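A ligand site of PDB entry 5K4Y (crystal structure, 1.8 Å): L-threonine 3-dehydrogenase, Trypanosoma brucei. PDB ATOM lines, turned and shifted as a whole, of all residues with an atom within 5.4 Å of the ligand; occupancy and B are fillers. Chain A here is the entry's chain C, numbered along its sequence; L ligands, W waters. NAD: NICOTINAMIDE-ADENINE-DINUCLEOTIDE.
O1N of the ligand is in hydrogen-bond range of N of Ile 13, at 3.0 Å.
OH of Tyr 143 lies within hydrogen-bond range of O2D of the ligand, at 2.7 Å.
N1A of the ligand is in hydrogen-bond range of N of Cys 55 (3.0 Å).
The side-chain amide oxygen (OE1) of Gln 12 is in hydrogen-bond range of a nitrogen (N7N) of the ligand (3.1 Å).
The side-chain amino group (NZ) of Lys 147 is in hydrogen-bond range of an oxygen (O3D) of the ligand.
The backbone carbonyl oxygen (O) of Leu 76 lies close to an oxygen (O3D) of the ligand.
OD2 of Asp 34 lies within hydrogen-bond range of O3B of the ligand (2.6 Å).
A nitrogen (N3A) of the ligand lies within hydrogen-bond range of the backbone NH (N) of Val 35 (3.5 Å).
OD1 of Asp 54 lies within hydrogen-bond range of N6A of the ligand.
The backbone NH of Gln 12 is in hydrogen-bond range of an oxygen (O1A) of the ligand (2.8 Å).
An oxygen (O3B) of the ligand lies within hydrogen-bond range of the backbone NH (N) of Gly 11, 3.2 Å away.
An oxygen (O7N) of the ligand lies within hydrogen-bond range of the backbone NH of Ile 173, at 3.1 Å.
The backbone NH (N) of Ala 9 is in hydrogen-bond range of the side-chain carboxylate (OD2) of Asp 34, at 3.3 Å.
The side-chain carboxylate of Asp 34 sits at hydrogen-bond distance from the backbone NH of Leu 10, 3.1 Å away.
The backbone carbonyl oxygen of Pro 116 lies within hydrogen-bond range of the side-chain amino group of Lys 147, 2.9 Å away.
The backbone NH of Leu 56 lies within hydrogen-bond range of the side-chain carboxylate of Asp 54, 2.9 Å away.
O of Leu 170 lies within hydrogen-bond range of N of Ile 119.
O of Ile 94 is in hydrogen-bond range of OG1 of Thr 98 (2.6 Å).
The side-chain amide nitrogen of Gln 12 sits at hydrogen-bond distance from the backbone carbonyl oxygen of Ile 173 (2.9 Å).
The backbone carbonyl oxygen of Asp 34 lies within hydrogen-bond range of the backbone NH of Leu 53.
An oxygen (O2N) of the ligand sits close to the side-chain sulfur (SD) of Met 80 (3.7 Å).
Gly 8 touches the ligand.
Leu 10 touches the ligand (C to O3B, 3.6 Å).
O of Leu 53 touches C2A of the ligand (3.4 Å).
Pro 77 touches the ligand (CB to C4A, 3.5 Å).
CB of Ala 78 touches O3D of the ligand (3.4 Å).
Ile 94 touches the ligand.
Pro 116 touches the ligand (CG to O3D, 3.4 Å).
Ser 117 touches the ligand (O to C6N, 3.3 Å).
Thr 118 touches the ligand.
CB of Leu 170 touches C5N of the ligand, 3.4 Å away.
Pro 171 touches the ligand (O to C4N, 3.3 Å).
Gly 172 touches the ligand.
Within 4 Å of the ligand: Gly 8, Leu 10, Gly 11, Gln 12, Ile 13, Asp 34, Val 35, Leu 53, Asp 54, Cys 55, Leu 76, Pro 77, Ala 78, Met 80, Ile 94, Pro 116, Ser 117, Thr 118, Tyr 143, Lys 147, Leu 170, Pro 171, Gly 172 and Ile 173.
Water W9 bridges an oxygen (O2N) of the ligand and the side-chain amide oxygen (OE1) of Gln 12.
Water W11 lies within hydrogen-bond range of O1N of the ligand, O of Gly 8, N of Gly 14 and N of Gly 11.
Water W6 bridges OG1 of Thr 185 and O7N of the ligand.
Water W1 lies within hydrogen-bond range of O of Leu 53, N of Asp 34, N of Gly 8 and SG of Cys 55.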
ATOM      1  N   THR A   7      11.940   8.986   9.741  1.00  0.00           N
ATOM      2  CA  THR A   7      12.593   9.475  10.956  1.00  0.00           C
ATOM      3  C   THR A   7      12.344   8.505  12.149  1.00  0.00           C
ATOM      4  O   THR A   7      11.369   7.741  12.135  1.00  0.00           O
ATOM      5  CB  THR A   7      12.096  10.873  11.322  1.00  0.00           C
ATOM      6  OG1 THR A   7      10.674  10.796  11.612  1.00  0.00           O
ATOM      7  CG2 THR A   7      12.400  11.938  10.226  1.00  0.00           C
ATOM      8  N   GLY A   8      13.207   8.542  13.157  1.00  0.00           N
ATOM      9  CA  GLY A   8      13.293   7.463  14.136  1.00  0.00           C
ATOM     10  C   GLY A   8      13.354   6.064  13.516  1.00  0.00           C
ATOM     11  O   GLY A   8      12.668   5.154  13.906  1.00  0.00           O
ATOM     12  N   ALA A   9      14.127   5.955  12.443  1.00  0.00           N
ATOM     13  CA  ALA A   9      14.104   4.784  11.590  1.00  0.00           C
ATOM     14  C   ALA A   9      14.864   3.584  12.052  1.00  0.00           C
ATOM     15  O   ALA A   9      14.733   2.522  11.454  1.00  0.00           O
ATOM     16  CB  ALA A   9      14.600   5.151  10.204  1.00  0.00           C
ATOM     17  N   LEU A  10      15.644   3.702  13.102  1.00  0.00           N
ATOM     18  CA  LEU A  10      16.441   2.560  13.596  1.00  0.00           C
ATOM     19  C   LEU A  10      15.869   1.718  14.713  1.00  0.00           C
ATOM     20  O   LEU A  10      16.529   0.772  15.156  1.00  0.00           O
ATOM     21  CB  LEU A  10      17.842   3.085  14.016  1.00  0.00           C
ATOM     22  CG  LEU A  10      18.661   3.711  12.936  1.00  0.00           C
ATOM     23  CD1 LEU A  10      20.134   3.920  13.356  1.00  0.00           C
ATOM     24  CD2 LEU A  10      18.575   2.940  11.650  1.00  0.00           C
ATOM     25  N   GLY A  11      14.647   1.982  15.145  1.00  0.00           N
ATOM     26  CA  GLY A  11      13.970   1.260  16.165  1.00  0.00           C
ATOM     27  C   GLY A  11      13.292   0.025  15.616  1.00  0.00           C
ATOM     28  O   GLY A  11      13.633  -0.445  14.498  1.00  0.00           O
ATOM     29  N   GLN A  12      12.257  -0.426  16.302  1.00  0.00           N
ATOM     30  CA  GLN A  12      11.654  -1.736  16.043  1.00  0.00           C
ATOM     31  C   GLN A  12      10.926  -1.701  14.713  1.00  0.00           C
ATOM     32  O   GLN A  12      11.227  -2.539  13.810  1.00  0.00           O
ATOM     33  CB  GLN A  12      10.700  -2.154  17.116  1.00  0.00           C
ATOM     34  CG  GLN A  12       9.999  -3.517  16.842  1.00  0.00           C
ATOM     35  CD  GLN A  12       8.874  -3.937  17.776  1.00  0.00           C
ATOM     36  OE1 GLN A  12       8.473  -3.252  18.701  1.00  0.00           O
ATOM     37  NE2 GLN A  12       8.345  -5.111  17.511  1.00  0.00           N
ATOM     38  N   ILE A  13      10.001  -0.743  14.570  1.00  0.00           N
ATOM     39  CA  ILE A  13       9.243  -0.623  13.298  1.00  0.00           C
ATOM     40  C   ILE A  13      10.136  -0.060  12.217  1.00  0.00           C
ATOM     41  O   ILE A  13      10.087  -0.508  11.085  1.00  0.00           O
ATOM     42  CB  ILE A  13       7.997   0.281  13.512  1.00  0.00           C
ATOM     43  CG1 ILE A  13       7.069  -0.448  14.508  1.00  0.00           C
ATOM     44  CG2 ILE A  13       7.348   0.714  12.187  1.00  0.00           C
ATOM     45  CD1 ILE A  13       5.949   0.362  14.955  1.00  0.00           C
ATOM     46  N   GLY A  14      10.924   0.970  12.509  1.00  0.00           N
ATOM     47  CA  GLY A  14      11.683   1.656  11.502  1.00  0.00           C
ATOM     48  C   GLY A  14      12.715   0.777  10.765  1.00  0.00           C
ATOM     49  O   GLY A  14      12.909   0.942   9.569  1.00  0.00           O
ATOM     50  N   ASP A  34      17.779   8.809  12.078  1.00  0.00           N
ATOM     51  CA  ASP A  34      17.547   8.559  13.493  1.00  0.00           C
ATOM     52  C   ASP A  34      18.520   9.404  14.307  1.00  0.00           C
ATOM     53  O   ASP A  34      19.557   9.794  13.806  1.00  0.00           O
ATOM     54  CB  ASP A  34      17.692   7.072  13.852  1.00  0.00           C
ATOM     55  CG  ASP A  34      17.019   6.701  15.189  1.00  0.00           C
ATOM     56  OD1 ASP A  34      17.520   7.109  16.258  1.00  0.00           O
ATOM     57  OD2 ASP A  34      16.041   5.953  15.146  1.00  0.00           O
ATOM     58  N   VAL A  35      18.204   9.676  15.565  1.00  0.00           N
ATOM     59  CA  VAL A  35      19.090  10.420  16.449  1.00  0.00           C
ATOM     60  C   VAL A  35      20.366   9.616  16.766  1.00  0.00           C
ATOM     61  O   VAL A  35      21.474  10.190  17.084  1.00  0.00           O
ATOM     62  CB  VAL A  35      18.361  10.911  17.694  1.00  0.00           C
ATOM     63  CG1 VAL A  35      17.976   9.828  18.648  1.00  0.00           C
ATOM     64  CG2 VAL A  35      19.147  11.951  18.412  1.00  0.00           C
ATOM     65  N   VAL A  36      20.213   8.309  16.723  1.00  0.00           N
ATOM     66  CA  VAL A  36      21.387   7.420  16.899  1.00  0.00           C
ATOM     67  C   VAL A  36      21.871   6.831  15.598  1.00  0.00           C
ATOM     68  O   VAL A  36      21.176   6.901  14.599  1.00  0.00           O
ATOM     69  CB  VAL A  36      21.164   6.298  17.934  1.00  0.00           C
ATOM     70  CG1 VAL A  36      20.797   6.867  19.284  1.00  0.00           C
ATOM     71  CG2 VAL A  36      20.155   5.265  17.469  1.00  0.00           C
ATOM     72  N   LEU A  53      19.959  12.339  12.627  1.00  0.00           N
ATOM     73  CA  LEU A  53      19.142  13.564  12.739  1.00  0.00           C
ATOM     74  C   LEU A  53      18.393  13.523  14.059  1.00  0.00           C
ATOM     75  O   LEU A  53      17.646  12.552  14.274  1.00  0.00           O
ATOM     76  CB  LEU A  53      18.112  13.645  11.629  1.00  0.00           C
ATOM     77  CG  LEU A  53      17.056  14.752  11.804  1.00  0.00           C
ATOM     78  CD1 LEU A  53      17.596  16.184  11.798  1.00  0.00           C
ATOM     79  CD2 LEU A  53      15.929  14.565  10.773  1.00  0.00           C
ATOM     80  N   ASP A  54      18.647  14.522  14.904  1.00  0.00           N
ATOM     81  CA  ASP A  54      17.803  14.768  16.118  1.00  0.00           C
ATOM     82  C   ASP A  54      16.564  15.634  15.660  1.00  0.00           C
ATOM     83  O   ASP A  54      16.727  16.788  15.301  1.00  0.00           O
ATOM     84  CB  ASP A  54      18.592  15.503  17.174  1.00  0.00           C
ATOM     85  CG  ASP A  54      17.844  15.633  18.474  1.00  0.00           C
ATOM     86  OD1 ASP A  54      16.587  15.391  18.486  1.00  0.00           O
ATOM     87  OD2 ASP A  54      18.512  15.920  19.464  1.00  0.00           O
ATOM     88  N   CYS A  55      15.389  15.002  15.653  1.00  0.00           N
ATOM     89  CA  CYS A  55      14.163  15.710  15.237  1.00  0.00           C
ATOM     90  C   CYS A  55      13.757  16.828  16.165  1.00  0.00           C
ATOM     91  O   CYS A  55      12.839  17.568  15.844  1.00  0.00           O
ATOM     92  CB  CYS A  55      12.965  14.719  15.002  1.00  0.00           C
ATOM     93  SG  CYS A  55      13.226  13.674  13.523  1.00  0.00           S
ATOM     94  N   LEU A  56      14.391  16.963  17.315  1.00  0.00           N
ATOM     95  CA  LEU A  56      14.159  18.157  18.167  1.00  0.00           C
ATOM     96  C   LEU A  56      14.872  19.366  17.624  1.00  0.00           C
ATOM     97  O   LEU A  56      14.556  20.472  18.033  1.00  0.00           O
ATOM     98  CB  LEU A  56      14.582  17.893  19.582  1.00  0.00           C
ATOM     99  CG  LEU A  56      13.689  16.932  20.371  1.00  0.00           C
ATOM    100  CD1 LEU A  56      14.330  16.541  21.710  1.00  0.00           C
ATOM    101  CD2 LEU A  56      12.339  17.598  20.617  1.00  0.00           C
ATOM    102  N   HIS A  75       7.022   9.487  10.172  1.00  0.00           N
ATOM    103  CA  HIS A  75       7.638  10.055  11.352  1.00  0.00           C
ATOM    104  C   HIS A  75       7.463   9.164  12.573  1.00  0.00           C
ATOM    105  O   HIS A  75       6.411   9.167  13.221  1.00  0.00           O
ATOM    106  CB  HIS A  75       7.044  11.496  11.623  1.00  0.00           C
ATOM    107  CG  HIS A  75       7.669  12.158  12.786  1.00  0.00           C
ATOM    108  ND1 HIS A  75       8.968  12.674  12.761  1.00  0.00           N
ATOM    109  CD2 HIS A  75       7.232  12.339  14.052  1.00  0.00           C
ATOM    110  CE1 HIS A  75       9.247  13.195  13.934  1.00  0.00           C
ATOM    111  NE2 HIS A  75       8.187  13.031  14.723  1.00  0.00           N
ATOM    112  N   LEU A  76       8.506   8.386  12.901  1.00  0.00           N
ATOM    113  CA  LEU A  76       8.408   7.371  13.962  1.00  0.00           C
ATOM    114  C   LEU A  76       8.896   7.640  15.418  1.00  0.00           C
ATOM    115  O   LEU A  76       8.545   6.817  16.255  1.00  0.00           O
ATOM    116  CB  LEU A  76       9.051   6.047  13.447  1.00  0.00           C
ATOM    117  CG  LEU A  76       8.584   5.551  12.056  1.00  0.00           C
ATOM    118  CD1 LEU A  76       9.344   4.312  11.593  1.00  0.00           C
ATOM    119  CD2 LEU A  76       7.095   5.226  12.026  1.00  0.00           C
ATOM    120  N   PRO A  77       9.623   8.709  15.709  1.00  0.00           N
ATOM    121  CA  PRO A  77      10.156   8.721  17.036  1.00  0.00           C
ATOM    122  C   PRO A  77       9.056   8.985  18.066  1.00  0.00           C
ATOM    123  O   PRO A  77       8.242   9.849  17.841  1.00  0.00           O
ATOM    124  CB  PRO A  77      11.121   9.900  17.040  1.00  0.00           C
ATOM    125  CG  PRO A  77      10.934  10.602  15.823  1.00  0.00           C
ATOM    126  CD  PRO A  77      10.107   9.837  14.891  1.00  0.00           C
ATOM    127  N   ALA A  78       9.105   8.258  19.166  1.00  0.00           N
ATOM    128  CA  ALA A  78       8.207   8.447  20.298  1.00  0.00           C
ATOM    129  C   ALA A  78       8.798   7.765  21.505  1.00  0.00           C
ATOM    130  O   ALA A  78       9.683   6.933  21.377  1.00  0.00           O
ATOM    131  CB  ALA A  78       6.828   7.858  20.053  1.00  0.00           C
ATOM    132  N   MET A  80       7.414   5.543  24.492  1.00  0.00           N
ATOM    133  CA  MET A  80       6.182   4.776  24.584  1.00  0.00           C
ATOM    134  C   MET A  80       5.721   4.615  26.068  1.00  0.00           C
ATOM    135  O   MET A  80       6.209   5.352  26.934  1.00  0.00           O
ATOM    136  CB  MET A  80       6.367   3.480  23.806  1.00  0.00           C
ATOM    137  CG  MET A  80       6.529   3.755  22.286  1.00  0.00           C
ATOM    138  SD  MET A  80       6.985   2.253  21.367  1.00  0.00           S
ATOM    139  CE  MET A  80       5.618   1.200  21.735  1.00  0.00           C
ATOM    140  N   ILE A  94       9.571  14.841  23.021  1.00  0.00           N
ATOM    141  CA  ILE A  94       9.686  14.092  21.817  1.00  0.00           C
ATOM    142  C   ILE A  94       8.307  13.931  21.109  1.00  0.00           C
ATOM    143  O   ILE A  94       8.189  14.203  19.886  1.00  0.00           O
ATOM    144  CB  ILE A  94      10.323  12.688  22.060  1.00  0.00           C
ATOM    145  CG1 ILE A  94      11.766  12.805  22.516  1.00  0.00           C
ATOM    146  CG2 ILE A  94      10.260  11.828  20.826  1.00  0.00           C
ATOM    147  CD1 ILE A  94      12.611  13.574  21.558  1.00  0.00           C
ATOM    148  N   THR A  98       8.598  16.932  18.305  1.00  0.00           N
ATOM    149  CA  THR A  98       9.048  16.444  17.024  1.00  0.00           C
ATOM    150  C   THR A  98       7.932  16.367  16.017  1.00  0.00           C
ATOM    151  O   THR A  98       8.116  16.574  14.836  1.00  0.00           O
ATOM    152  CB  THR A  98       9.789  15.108  17.104  1.00  0.00           C
ATOM    153  OG1 THR A  98       8.935  14.008  17.404  1.00  0.00           O
ATOM    154  CG2 THR A  98      10.935  15.212  18.086  1.00  0.00           C
ATOM    155  N   PRO A 116       2.300   7.320  13.250  1.00  0.00           N
ATOM    156  CA  PRO A 116       1.523   6.284  13.818  1.00  0.00           C
ATOM    157  C   PRO A 116       0.886   6.754  15.161  1.00  0.00           C
ATOM    158  O   PRO A 116       1.523   7.483  15.928  1.00  0.00           O
ATOM    159  CB  PRO A 116       2.569   5.203  14.120  1.00  0.00           C
ATOM    160  CG  PRO A 116       3.830   5.936  14.270  1.00  0.00           C
ATOM    161  CD  PRO A 116       3.728   7.037  13.312  1.00  0.00           C
ATOM    162  N   SER A 117      -0.368   6.354  15.377  1.00  0.00           N
ATOM    163  CA  SER A 117      -0.950   6.420  16.715  1.00  0.00           C
ATOM    164  C   SER A 117      -0.891   5.007  17.307  1.00  0.00           C
ATOM    165  O   SER A 117      -0.019   4.178  16.905  1.00  0.00           O
ATOM    166  CB  SER A 117      -2.327   7.102  16.768  1.00  0.00           C
ATOM    167  OG  SER A 117      -2.820   7.183  18.107  1.00  0.00           O
ATOM    168  N   THR A 118      -1.748   4.714  18.273  1.00  0.00           N
ATOM    169  CA  THR A 118      -1.607   3.540  19.084  1.00  0.00           C
ATOM    170  C   THR A 118      -2.884   3.236  19.825  1.00  0.00           C
ATOM    171  O   THR A 118      -3.677   4.129  20.132  1.00  0.00           O
ATOM    172  CB  THR A 118      -0.455   3.676  20.121  1.00  0.00           C
ATOM    173  OG1 THR A 118      -0.495   2.581  21.036  1.00  0.00           O
ATOM    174  CG2 THR A 118      -0.586   4.939  20.870  1.00  0.00           C
ATOM    175  N   ILE A 119      -3.113   1.947  20.091  1.00  0.00           N
ATOM    176  CA  ILE A 119      -4.184   1.558  20.993  1.00  0.00           C
ATOM    177  C   ILE A 119      -4.025   2.144  22.386  1.00  0.00           C
ATOM    178  O   ILE A 119      -5.039   2.251  23.101  1.00  0.00           O
ATOM    179  CB  ILE A 119      -4.334   0.029  21.157  1.00  0.00           C
ATOM    180  CG1 ILE A 119      -3.079  -0.586  21.738  1.00  0.00           C
ATOM    181  CG2 ILE A 119      -4.763  -0.604  19.834  1.00  0.00           C
ATOM    182  CD1 ILE A 119      -3.208  -2.079  22.110  1.00  0.00           C
ATOM    183  N   TYR A 143       2.058   8.907  27.406  1.00  0.00           N
ATOM    184  CA  TYR A 143       2.264   8.559  26.027  1.00  0.00           C
ATOM    185  C   TYR A 143       0.941   8.603  25.248  1.00  0.00           C
ATOM    186  O   TYR A 143       0.787   9.238  24.198  1.00  0.00           O
ATOM    187  CB  TYR A 143       2.794   7.131  26.005  1.00  0.00           C
ATOM    188  CG  TYR A 143       2.742   6.363  24.702  1.00  0.00           C
ATOM    189  CD1 TYR A 143       3.362   6.839  23.544  1.00  0.00           C
ATOM    190  CD2 TYR A 143       2.198   5.046  24.651  1.00  0.00           C
ATOM    191  CE1 TYR A 143       3.422   6.050  22.371  1.00  0.00           C
ATOM    192  CE2 TYR A 143       2.275   4.287  23.523  1.00  0.00           C
ATOM    193  CZ  TYR A 143       2.892   4.759  22.395  1.00  0.00           C
ATOM    194  OH  TYR A 143       2.967   3.932  21.299  1.00  0.00           O
ATOM    195  N   LYS A 147      -0.483  10.998  22.126  1.00  0.00           N
ATOM    196  CA  LYS A 147      -0.853  10.461  20.821  1.00  0.00           C
ATOM    197  C   LYS A 147      -2.271  10.919  20.418  1.00  0.00           C
ATOM    198  O   LYS A 147      -2.540  11.113  19.232  1.00  0.00           O
ATOM    199  CB  LYS A 147      -0.759   8.972  20.800  1.00  0.00           C
ATOM    200  CG  LYS A 147       0.684   8.478  20.766  1.00  0.00           C
ATOM    201  CD  LYS A 147       1.427   8.754  19.505  1.00  0.00           C
ATOM    202  CE  LYS A 147       2.783   8.025  19.383  1.00  0.00           C
ATOM    203  NZ  LYS A 147       3.340   8.117  18.031  1.00  0.00           N
ATOM    204  N   LEU A 170      -1.810   1.669  15.881  1.00  0.00           N
ATOM    205  CA  LEU A 170      -1.153   0.356  15.894  1.00  0.00           C
ATOM    206  C   LEU A 170      -1.420  -0.375  17.217  1.00  0.00           C
ATOM    207  O   LEU A 170      -1.383   0.238  18.327  1.00  0.00           O
ATOM    208  CB  LEU A 170       0.332   0.485  15.698  1.00  0.00           C
ATOM    209  CG  LEU A 170       0.918   0.908  14.328  1.00  0.00           C
ATOM    210  CD1 LEU A 170       2.379   1.038  14.524  1.00  0.00           C
ATOM    211  CD2 LEU A 170       0.582  -0.095  13.253  1.00  0.00           C
ATOM    212  N   PRO A 171      -1.728  -1.681  17.119  1.00  0.00           N
ATOM    213  CA  PRO A 171      -1.740  -2.567  18.274  1.00  0.00           C
ATOM    214  C   PRO A 171      -0.322  -2.947  18.718  1.00  0.00           C
ATOM    215  O   PRO A 171       0.663  -2.390  18.202  1.00  0.00           O
ATOM    216  CB  PRO A 171      -2.522  -3.768  17.709  1.00  0.00           C
ATOM    217  CG  PRO A 171      -2.051  -3.839  16.278  1.00  0.00           C
ATOM    218  CD  PRO A 171      -1.846  -2.416  15.864  1.00  0.00           C
ATOM    219  N   GLY A 172      -0.186  -3.912  19.614  1.00  0.00           N
ATOM    220  CA  GLY A 172       1.161  -4.379  19.939  1.00  0.00           C
ATOM    221  C   GLY A 172       1.776  -5.032  18.734  1.00  0.00           C
ATOM    222  O   GLY A 172       1.131  -5.852  18.167  1.00  0.00           O
ATOM    223  N   ILE A 173       3.007  -4.700  18.386  1.00  0.00           N
ATOM    224  CA  ILE A 173       3.662  -5.219  17.191  1.00  0.00           C
ATOM    225  C   ILE A 173       4.760  -6.202  17.652  1.00  0.00           C
ATOM    226  O   ILE A 173       5.658  -5.844  18.480  1.00  0.00           O
ATOM    227  CB  ILE A 173       4.289  -4.071  16.380  1.00  0.00           C
ATOM    228  CG1 ILE A 173       3.299  -2.955  16.017  1.00  0.00           C
ATOM    229  CG2 ILE A 173       4.947  -4.598  15.093  1.00  0.00           C
ATOM    230  CD1 ILE A 173       2.016  -3.472  15.386  1.00  0.00           C
ATOM    231  N   THR A 185       4.252  -4.588  25.775  1.00  0.00           N
ATOM    232  CA  THR A 185       3.970  -5.876  25.155  1.00  0.00           C
ATOM    233  C   THR A 185       5.166  -6.768  24.958  1.00  0.00           C
ATOM    234  O   THR A 185       5.030  -7.767  24.236  1.00  0.00           O
ATOM    235  CB  THR A 185       3.167  -5.738  23.851  1.00  0.00           C
ATOM    236  OG1 THR A 185       3.923  -4.979  22.923  1.00  0.00           O
ATOM    237  CG2 THR A 185       1.838  -5.101  24.115  1.00  0.00           C
HETATM  238  PA  NAD L   1      11.386   2.316  19.114  1.00  0.00           P
HETATM  239  O1A NAD L   1      11.870   0.883  18.793  1.00  0.00           O
HETATM  240  O2A NAD L   1      11.528   2.823  20.576  1.00  0.00           O
HETATM  241  O5B NAD L   1      12.097   3.291  18.097  1.00  0.00           O
HETATM  242  C5B NAD L   1      12.067   4.661  18.221  1.00  0.00           C
HETATM  243  C4B NAD L   1      13.228   5.306  17.469  1.00  0.00           C
HETATM  244  O4B NAD L   1      12.974   6.712  17.657  1.00  0.00           O
HETATM  245  C3B NAD L   1      14.541   5.005  18.155  1.00  0.00           C
HETATM  246  O3B NAD L   1      15.408   4.421  17.114  1.00  0.00           O
HETATM  247  C2B NAD L   1      14.986   6.344  18.746  1.00  0.00           C
HETATM  248  O2B NAD L   1      16.463   6.431  18.635  1.00  0.00           O
HETATM  249  C1B NAD L   1      14.275   7.299  17.783  1.00  0.00           C
HETATM  250  N9A NAD L   1      14.294   8.674  18.337  1.00  0.00           N
HETATM  251  C8A NAD L   1      14.089   9.011  19.654  1.00  0.00           C
HETATM  252  N7A NAD L   1      14.221  10.338  19.818  1.00  0.00           N
HETATM  253  C5A NAD L   1      14.492  10.783  18.563  1.00  0.00           C
HETATM  254  C6A NAD L   1      14.759  12.051  18.086  1.00  0.00           C
HETATM  255  N6A NAD L   1      14.838  13.039  18.993  1.00  0.00           N
HETATM  256  N1A NAD L   1      15.019  12.243  16.788  1.00  0.00           N
HETATM  257  C2A NAD L   1      15.024  11.234  15.926  1.00  0.00           C
HETATM  258  N3A NAD L   1      14.825   9.979  16.392  1.00  0.00           N
HETATM  259  C4A NAD L   1      14.543   9.776  17.666  1.00  0.00           C
HETATM  260  O3  NAD L   1       9.832   2.504  18.735  1.00  0.00           O
HETATM  261  PN  NAD L   1       8.980   1.663  17.660  1.00  0.00           P
HETATM  262  O1N NAD L   1       9.747   1.538  16.433  1.00  0.00           O
HETATM  263  O2N NAD L   1       8.392   0.530  18.437  1.00  0.00           O
HETATM  264  O5D NAD L   1       7.721   2.679  17.442  1.00  0.00           O
HETATM  265  C5D NAD L   1       7.744   3.575  16.339  1.00  0.00           C
HETATM  266  C4D NAD L   1       6.433   4.415  16.266  1.00  0.00           C
HETATM  267  O4D NAD L   1       5.425   3.412  16.300  1.00  0.00           O
HETATM  268  C3D NAD L   1       6.232   5.241  17.541  1.00  0.00           C
HETATM  269  O3D NAD L   1       5.452   6.442  17.249  1.00  0.00           O
HETATM  270  C2D NAD L   1       5.296   4.362  18.427  1.00  0.00           C
HETATM  271  O2D NAD L   1       4.460   5.126  19.331  1.00  0.00           O
HETATM  272  C1D NAD L   1       4.487   3.671  17.395  1.00  0.00           C
HETATM  273  N1N NAD L   1       3.924   2.388  17.853  1.00  0.00           N
HETATM  274  C2N NAD L   1       4.760   1.281  18.040  1.00  0.00           C
HETATM  275  C3N NAD L   1       4.173   0.136  18.542  1.00  0.00           C
HETATM  276  C7N NAD L   1       4.976  -1.099  18.802  1.00  0.00           C
HETATM  277  O7N NAD L   1       4.360  -2.127  19.356  1.00  0.00           O
HETATM  278  N7N NAD L   1       6.274  -1.100  18.440  1.00  0.00           N
HETATM  279  C4N NAD L   1       2.807   0.094  18.771  1.00  0.00           C
HETATM  280  C5N NAD L   1       1.966   1.176  18.549  1.00  0.00           C
HETATM  281  C6N NAD L   1       2.503   2.333  18.064  1.00  0.00           C
HETATM  282  O   HOH W   1      15.443  11.041  12.603  1.00  0.00           O
HETATM  283  O   HOH W   2      17.331   7.139  20.909  1.00  0.00           O
HETATM  284  O   HOH W   3      13.414   3.849  21.752  1.00  0.00           O
HETATM  285  O   HOH W   4       5.973   8.906  15.951  1.00  0.00           O
HETATM  286  O   HOH W   5      17.201   2.694  18.289  1.00  0.00           O
HETATM  287  O   HOH W   6       3.946  -2.420  22.398  1.00  0.00           O
HETATM  288  O   HOH W   7      14.768  10.430  22.756  1.00  0.00           O
HETATM  289  O   HOH W   8      16.337  12.805  21.678  1.00  0.00           O
HETATM  290  O   HOH W   9       9.263  -0.885  20.533  1.00  0.00           O
HETATM  291  O   HOH W  10      13.774  -0.546  19.802  1.00  0.00           O
HETATM  292  O   HOH W  11      11.553   2.647  14.758  1.00  0.00           O
